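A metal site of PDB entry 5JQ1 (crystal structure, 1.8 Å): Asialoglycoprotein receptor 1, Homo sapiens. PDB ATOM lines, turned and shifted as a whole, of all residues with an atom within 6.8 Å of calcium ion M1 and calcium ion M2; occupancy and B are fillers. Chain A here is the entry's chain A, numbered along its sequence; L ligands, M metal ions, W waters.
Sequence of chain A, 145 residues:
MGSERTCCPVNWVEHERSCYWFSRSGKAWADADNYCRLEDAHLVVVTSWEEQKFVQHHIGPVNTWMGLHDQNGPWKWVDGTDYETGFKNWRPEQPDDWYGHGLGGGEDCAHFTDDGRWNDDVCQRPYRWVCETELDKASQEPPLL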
ATOM      1  N   ASP A  70      25.176  15.007  25.066  1.00  0.00           N
ATOM      2  CA  ASP A  70      24.549  14.016  25.947  1.00  0.00           C
ATOM      3  C   ASP A  70      23.168  13.644  25.397  1.00  0.00           C
ATOM      4  O   ASP A  70      22.248  13.326  26.156  1.00  0.00           O
ATOM      5  CB  ASP A  70      24.461  14.538  27.419  1.00  0.00           C
ATOM      6  CG  ASP A  70      23.415  15.599  27.685  1.00  0.00           C
ATOM      7  OD1 ASP A  70      23.022  16.307  26.731  1.00  0.00           O
ATOM      8  OD2 ASP A  70      22.999  15.746  28.853  1.00  0.00           O
ATOM      9  N   GLN A  71      23.055  13.627  24.057  1.00  0.00           N
ATOM     10  CA  GLN A  71      21.802  13.270  23.382  1.00  0.00           C
ATOM     11  C   GLN A  71      21.307  11.853  23.692  1.00  0.00           C
ATOM     12  O   GLN A  71      20.105  11.637  23.649  1.00  0.00           O
ATOM     13  CB  GLN A  71      21.884  13.470  21.857  1.00  0.00           C
ATOM     14  CG  GLN A  71      22.224  14.889  21.451  1.00  0.00           C
ATOM     15  CD  GLN A  71      22.256  15.018  19.965  1.00  0.00           C
ATOM     16  OE1 GLN A  71      23.294  14.855  19.332  1.00  0.00           O
ATOM     17  NE2 GLN A  71      21.120  15.359  19.384  1.00  0.00           N
ATOM     18  N   GLY A  73      22.137  10.120  26.582  1.00  0.00           N
ATOM     19  CA  GLY A  73      22.200   9.909  28.024  1.00  0.00           C
ATOM     20  C   GLY A  73      23.376  10.613  28.624  1.00  0.00           C
ATOM     21  O   GLY A  73      23.282  11.797  28.955  1.00  0.00           O
ATOM     22  N   TRP A  75      27.253  12.293  28.938  1.00  0.00           N
ATOM     23  CA  TRP A  75      28.165  13.073  28.088  1.00  0.00           C
ATOM     24  C   TRP A  75      29.095  12.113  27.301  1.00  0.00           C
ATOM     25  O   TRP A  75      29.650  11.180  27.879  1.00  0.00           O
ATOM     26  CB  TRP A  75      29.009  14.052  28.932  1.00  0.00           C
ATOM     27  CG  TRP A  75      28.186  15.234  29.364  1.00  0.00           C
ATOM     28  CD1 TRP A  75      27.647  15.453  30.598  1.00  0.00           C
ATOM     29  CD2 TRP A  75      27.648  16.247  28.507  1.00  0.00           C
ATOM     30  NE1 TRP A  75      26.886  16.603  30.582  1.00  0.00           N
ATOM     31  CE2 TRP A  75      26.833  17.085  29.305  1.00  0.00           C
ATOM     32  CE3 TRP A  75      27.807  16.556  27.145  1.00  0.00           C
ATOM     33  CZ2 TRP A  75      26.148  18.195  28.766  1.00  0.00           C
ATOM     34  CZ3 TRP A  75      27.122  17.646  26.614  1.00  0.00           C
ATOM     35  CH2 TRP A  75      26.285  18.437  27.428  1.00  0.00           C
ATOM     36  N   GLU A  93      28.605  27.233  36.476  1.00  0.00           N
ATOM     37  CA  GLU A  93      27.167  26.931  36.472  1.00  0.00           C
ATOM     38  C   GLU A  93      26.754  26.125  35.225  1.00  0.00           C
ATOM     39  O   GLU A  93      25.564  25.940  34.995  1.00  0.00           O
ATOM     40  CB  GLU A  93      26.268  28.192  36.625  1.00  0.00           C
ATOM     41  CG  GLU A  93      26.502  28.999  37.898  1.00  0.00           C
ATOM     42  CD  GLU A  93      25.467  30.097  38.102  1.00  0.00           C
ATOM     43  OE1 GLU A  93      24.624  29.943  39.005  1.00  0.00           O
ATOM     44  OE2 GLU A  93      25.463  31.069  37.307  1.00  0.00           O
ATOM     45  N   GLN A  94      27.727  25.646  34.435  1.00  0.00           N
ATOM     46  CA  GLN A  94      27.415  24.772  33.301  1.00  0.00           C
ATOM     47  C   GLN A  94      28.030  23.377  33.552  1.00  0.00           C
ATOM     48  O   GLN A  94      29.033  23.279  34.268  1.00  0.00           O
ATOM     49  CB  GLN A  94      27.921  25.357  31.954  1.00  0.00           C
ATOM     50  CG  GLN A  94      27.389  26.752  31.612  1.00  0.00           C
ATOM     51  CD  GLN A  94      25.877  26.864  31.564  1.00  0.00           C
ATOM     52  OE1 GLN A  94      25.138  25.874  31.293  1.00  0.00           O
ATOM     53  NE2 GLN A  94      25.425  28.112  31.695  1.00  0.00           N
ATOM     54  N   PRO A  95      27.521  22.314  32.906  1.00  0.00           N
ATOM     55  CA  PRO A  95      26.311  22.272  32.059  1.00  0.00           C
ATOM     56  C   PRO A  95      25.064  22.331  32.951  1.00  0.00           C
ATOM     57  O   PRO A  95      25.110  21.911  34.122  1.00  0.00           O
ATOM     58  CB  PRO A  95      26.462  20.944  31.304  1.00  0.00           C
ATOM     59  CG  PRO A  95      27.275  20.047  32.235  1.00  0.00           C
ATOM     60  CD  PRO A  95      28.100  20.960  33.118  1.00  0.00           C
ATOM     61  N   ASP A  96      23.960  22.841  32.444  1.00  0.00           N
ATOM     62  CA  ASP A  96      22.769  22.949  33.290  1.00  0.00           C
ATOM     63  C   ASP A  96      21.487  22.371  32.668  1.00  0.00           C
ATOM     64  O   ASP A  96      20.422  22.443  33.306  1.00  0.00           O
ATOM     65  CB  ASP A  96      22.578  24.412  33.716  1.00  0.00           C
ATOM     66  CG  ASP A  96      22.265  25.334  32.523  1.00  0.00           C
ATOM     67  OD1 ASP A  96      22.334  24.851  31.366  1.00  0.00           O
ATOM     68  OD2 ASP A  96      21.993  26.507  32.750  1.00  0.00           O
ATOM     69  N   ASP A  97      21.565  21.844  31.432  1.00  0.00           N
ATOM     70  CA  ASP A  97      20.414  21.267  30.700  1.00  0.00           C
ATOM     71  C   ASP A  97      19.175  22.181  30.760  1.00  0.00           C
ATOM     72  O   ASP A  97      18.087  21.747  31.137  1.00  0.00           O
ATOM     73  CB  ASP A  97      20.079  19.888  31.298  1.00  0.00           C
ATOM     74  CG  ASP A  97      19.232  18.983  30.412  1.00  0.00           C
ATOM     75  OD1 ASP A  97      19.489  18.914  29.187  1.00  0.00           O
ATOM     76  OD2 ASP A  97      18.294  18.353  30.944  1.00  0.00           O
ATOM     77  N   TRP A  98      19.377  23.469  30.528  1.00  0.00           N
ATOM     78  CA  TRP A  98      18.315  24.483  30.649  1.00  0.00           C
ATOM     79  C   TRP A  98      17.123  24.196  29.707  1.00  0.00           C
ATOM     80  O   TRP A  98      17.331  23.949  28.522  1.00  0.00           O
ATOM     81  CB  TRP A  98      18.919  25.880  30.374  1.00  0.00           C
ATOM     82  CG  TRP A  98      18.007  27.046  30.646  1.00  0.00           C
ATOM     83  CD1 TRP A  98      17.345  27.331  31.808  1.00  0.00           C
ATOM     84  CD2 TRP A  98      17.791  28.168  29.758  1.00  0.00           C
ATOM     85  NE1 TRP A  98      16.689  28.542  31.683  1.00  0.00           N
ATOM     86  CE2 TRP A  98      16.937  29.070  30.444  1.00  0.00           C
ATOM     87  CE3 TRP A  98      18.197  28.472  28.448  1.00  0.00           C
ATOM     88  CZ2 TRP A  98      16.529  30.284  29.861  1.00  0.00           C
ATOM     89  CZ3 TRP A  98      17.778  29.659  27.871  1.00  0.00           C
ATOM     90  CH2 TRP A  98      16.912  30.533  28.562  1.00  0.00           C
ATOM     91  N   GLY A 106      15.850  19.939  26.908  1.00  0.00           N
ATOM     92  CA  GLY A 106      16.853  20.652  27.700  1.00  0.00           C
ATOM     93  C   GLY A 106      17.936  21.215  26.783  1.00  0.00           C
ATOM     94  O   GLY A 106      17.632  21.967  25.841  1.00  0.00           O
ATOM     95  N   GLU A 107      19.191  20.894  27.059  1.00  0.00           N
ATOM     96  CA  GLU A 107      20.340  21.368  26.243  1.00  0.00           C
ATOM     97  C   GLU A 107      21.298  20.218  26.177  1.00  0.00           C
ATOM     98  O   GLU A 107      21.734  19.750  27.227  1.00  0.00           O
ATOM     99  CB  GLU A 107      21.011  22.564  26.913  1.00  0.00           C
ATOM    100  CG  GLU A 107      20.256  23.850  26.682  1.00  0.00           C
ATOM    101  CD  GLU A 107      20.812  25.014  27.447  1.00  0.00           C
ATOM    102  OE1 GLU A 107      20.582  26.163  26.996  1.00  0.00           O
ATOM    103  OE2 GLU A 107      21.475  24.793  28.490  1.00  0.00           O
ATOM    104  N   ASP A 108      21.577  19.699  24.961  1.00  0.00           N
ATOM    105  CA  ASP A 108      22.343  18.466  24.851  1.00  0.00           C
ATOM    106  C   ASP A 108      23.672  18.527  24.091  1.00  0.00           C
ATOM    107  O   ASP A 108      24.294  17.479  23.950  1.00  0.00           O
ATOM    108  CB  ASP A 108      21.431  17.382  24.205  1.00  0.00           C
ATOM    109  CG  ASP A 108      20.166  17.056  24.993  1.00  0.00           C
ATOM    110  OD1 ASP A 108      20.064  17.486  26.161  1.00  0.00           O
ATOM    111  OD2 ASP A 108      19.357  16.264  24.504  1.00  0.00           O
ATOM    112  N   CYS A 109      24.060  19.708  23.540  1.00  0.00           N
ATOM    113  CA  CYS A 109      25.244  19.850  22.698  1.00  0.00           C
ATOM    114  C   CYS A 109      26.228  20.865  23.275  1.00  0.00           C
ATOM    115  O   CYS A 109      25.829  21.949  23.668  1.00  0.00           O
ATOM    116  CB  CYS A 109      24.834  20.193  21.260  1.00  0.00           C
ATOM    117  SG  CYS A 109      24.027  18.830  20.371  1.00  0.00           S
ATOM    118  N   HIS A 111      29.337  23.615  23.254  1.00  0.00           N
ATOM    119  CA  HIS A 111      30.005  24.593  22.422  1.00  0.00           C
ATOM    120  C   HIS A 111      30.988  25.419  23.261  1.00  0.00           C
ATOM    121  O   HIS A 111      30.795  25.588  24.456  1.00  0.00           O
ATOM    122  CB  HIS A 111      28.981  25.523  21.682  1.00  0.00           C
ATOM    123  CG  HIS A 111      28.217  26.473  22.570  1.00  0.00           C
ATOM    124  ND1 HIS A 111      28.638  27.792  22.757  1.00  0.00           N
ATOM    125  CD2 HIS A 111      27.080  26.266  23.282  1.00  0.00           C
ATOM    126  CE1 HIS A 111      27.736  28.331  23.562  1.00  0.00           C
ATOM    127  NE2 HIS A 111      26.811  27.457  23.936  1.00  0.00           N
ATOM    128  N   ASN A 119      29.673  25.477  27.281  1.00  0.00           N
ATOM    129  CA  ASN A 119      28.265  25.561  27.619  1.00  0.00           C
ATOM    130  C   ASN A 119      27.518  24.457  26.893  1.00  0.00           C
ATOM    131  O   ASN A 119      27.899  24.106  25.793  1.00  0.00           O
ATOM    132  CB  ASN A 119      27.685  26.925  27.218  1.00  0.00           C
ATOM    133  CG  ASN A 119      26.209  27.031  27.518  1.00  0.00           C
ATOM    134  OD1 ASN A 119      25.750  26.637  28.585  1.00  0.00           O
ATOM    135  ND2 ASN A 119      25.425  27.327  26.504  1.00  0.00           N
ATOM    136  N   ASP A 120      26.440  23.929  27.493  1.00  0.00           N
ATOM    137  CA  ASP A 120      25.561  22.974  26.808  1.00  0.00           C
ATOM    138  C   ASP A 120      24.408  23.839  26.256  1.00  0.00           C
ATOM    139  O   ASP A 120      23.923  24.735  26.938  1.00  0.00           O
ATOM    140  CB  ASP A 120      25.021  21.884  27.750  1.00  0.00           C
ATOM    141  CG  ASP A 120      24.267  22.352  28.978  1.00  0.00           C
ATOM    142  OD1 ASP A 120      24.603  23.454  29.522  1.00  0.00           O
ATOM    143  OD2 ASP A 120      23.479  21.541  29.519  1.00  0.00           O
ATOM    144  N   ASP A 121      24.028  23.627  24.999  1.00  0.00           N
ATOM    145  CA  ASP A 121      22.963  24.414  24.367  1.00  0.00           C
ATOM    146  C   ASP A 121      22.085  23.509  23.525  1.00  0.00           C
ATOM    147  O   ASP A 121      22.348  22.320  23.353  1.00  0.00           O
ATOM    148  CB  ASP A 121      23.577  25.570  23.498  1.00  0.00           C
ATOM    149  CG  ASP A 121      22.735  26.829  23.441  1.00  0.00           C
ATOM    150  OD1 ASP A 121      21.500  26.735  23.614  1.00  0.00           O
ATOM    151  OD2 ASP A 121      23.329  27.944  23.335  1.00  0.00           O
HETATM  152  C1  LIG L   1      22.379  28.680  28.341  1.00  0.00           C
HETATM  153  C2  LIG L   1      20.958  30.995  29.542  1.00  0.00           C
HETATM  154  C3  LIG L   1      21.669  29.920  30.466  1.00  0.00           C
HETATM  155  C4  LIG L   1      21.076  29.754  31.895  1.00  0.00           C
HETATM  156  C5  LIG L   1      23.272  30.936  29.243  1.00  0.00           C
HETATM  157  O1  LIG L   1      25.974  30.471  27.198  1.00  0.00           O
HETATM  158  C6  LIG L   1      25.029  30.478  26.461  1.00  0.00           C
HETATM  159  C7  LIG L   1      25.095  30.906  25.001  1.00  0.00           C
HETATM  160  N1  LIG L   1      23.786  30.100  26.949  1.00  0.00           N
HETATM  161  C8  LIG L   1      23.559  29.676  28.328  1.00  0.00           C
HETATM  162  O2  LIG L   1      22.774  27.485  27.746  1.00  0.00           O
HETATM  163  C9  LIG L   1      21.796  28.507  29.775  1.00  0.00           C
HETATM  164  O3  LIG L   1      22.729  27.662  30.441  1.00  0.00           O
HETATM  165  O4  LIG L   1      21.202  30.918  32.627  1.00  0.00           O
HETATM  166  O5  LIG L   1      22.983  30.453  30.554  1.00  0.00           O
HETATM  167  O6  LIG L   1      22.072  31.597  28.841  1.00  0.00           O
HETATM  168 CA    CA M   1      21.364  17.577  28.366  1.00  0.00          CA
HETATM  169 CA    CA M   2      23.599  25.629  29.322  1.00  0.00          CA
HETATM  170  O   HOH W   1      21.205  16.623  30.833  1.00  0.00           O
HETATM  171  O   HOH W   2      22.928  18.869  29.684  1.00  0.00           O
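Within 4 Å of calcium ion M2: Gln 94, Asp 96, Glu 107, Asn 119 and Asp 120. The nearest printed residue that does not touch calcium ion M2 is Asp 121 (4.8 Å).
The backbone NH (N) of Asp 97 lies within hydrogen-bond range of the side-chain carboxylate (OD2) of Asp 120 (2.7 Å). OE2 of Glu 107 sits close to N of Trp 98 (3.2 Å). A ring nitrogen (NE2) of His 111 is in hydrogen-bond range of the side-chain amide nitrogen (ND2) of Asn 119 (2.9 Å). The backbone NH (N) of Trp 98 lies close to the side-chain carboxylate (OD1) of Asp 96 (3.4 Å). N of Asp 108 sits at hydrogen-bond distance from O of Asp 121, 3.2 Å away.
Of the 18 residues printed, 4 come within 4 Å of calcium ion M1.
Calcium ion M1 is bound by water W2 (2.4 Å), the side-chain carboxylate (OD1) of Asp 97 (2.4 Å), the backbone carbonyl oxygen (O) of Glu 107 (2.5 Å), the side-chain carboxylate (OD2) of Asp 70 (2.5 Å), the side-chain carboxylate (OD1) of Asp 108 (2.6 Å), water W1 (2.6 Å) and the side-chain carboxylate (OD1) of Asp 70 (2.7 Å). Calcium ion M1 has seven donor atoms within binding distance.
Calcium ion M2 is bound by OD1 of Asp 120 (2.4 Å), OE2 of Glu 107 (2.4 Å), O3 of the ligand (2.5 Å), OD1 of Asn 119 (2.5 Å), OE1 of Gln 94 (2.5 Å), OD1 of Asp 96 (2.5 Å), O of Asp 120 (2.6 Å) and O2 of the ligand (2.6 Å). Calcium ion M2 has eight donor atoms within binding distance.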
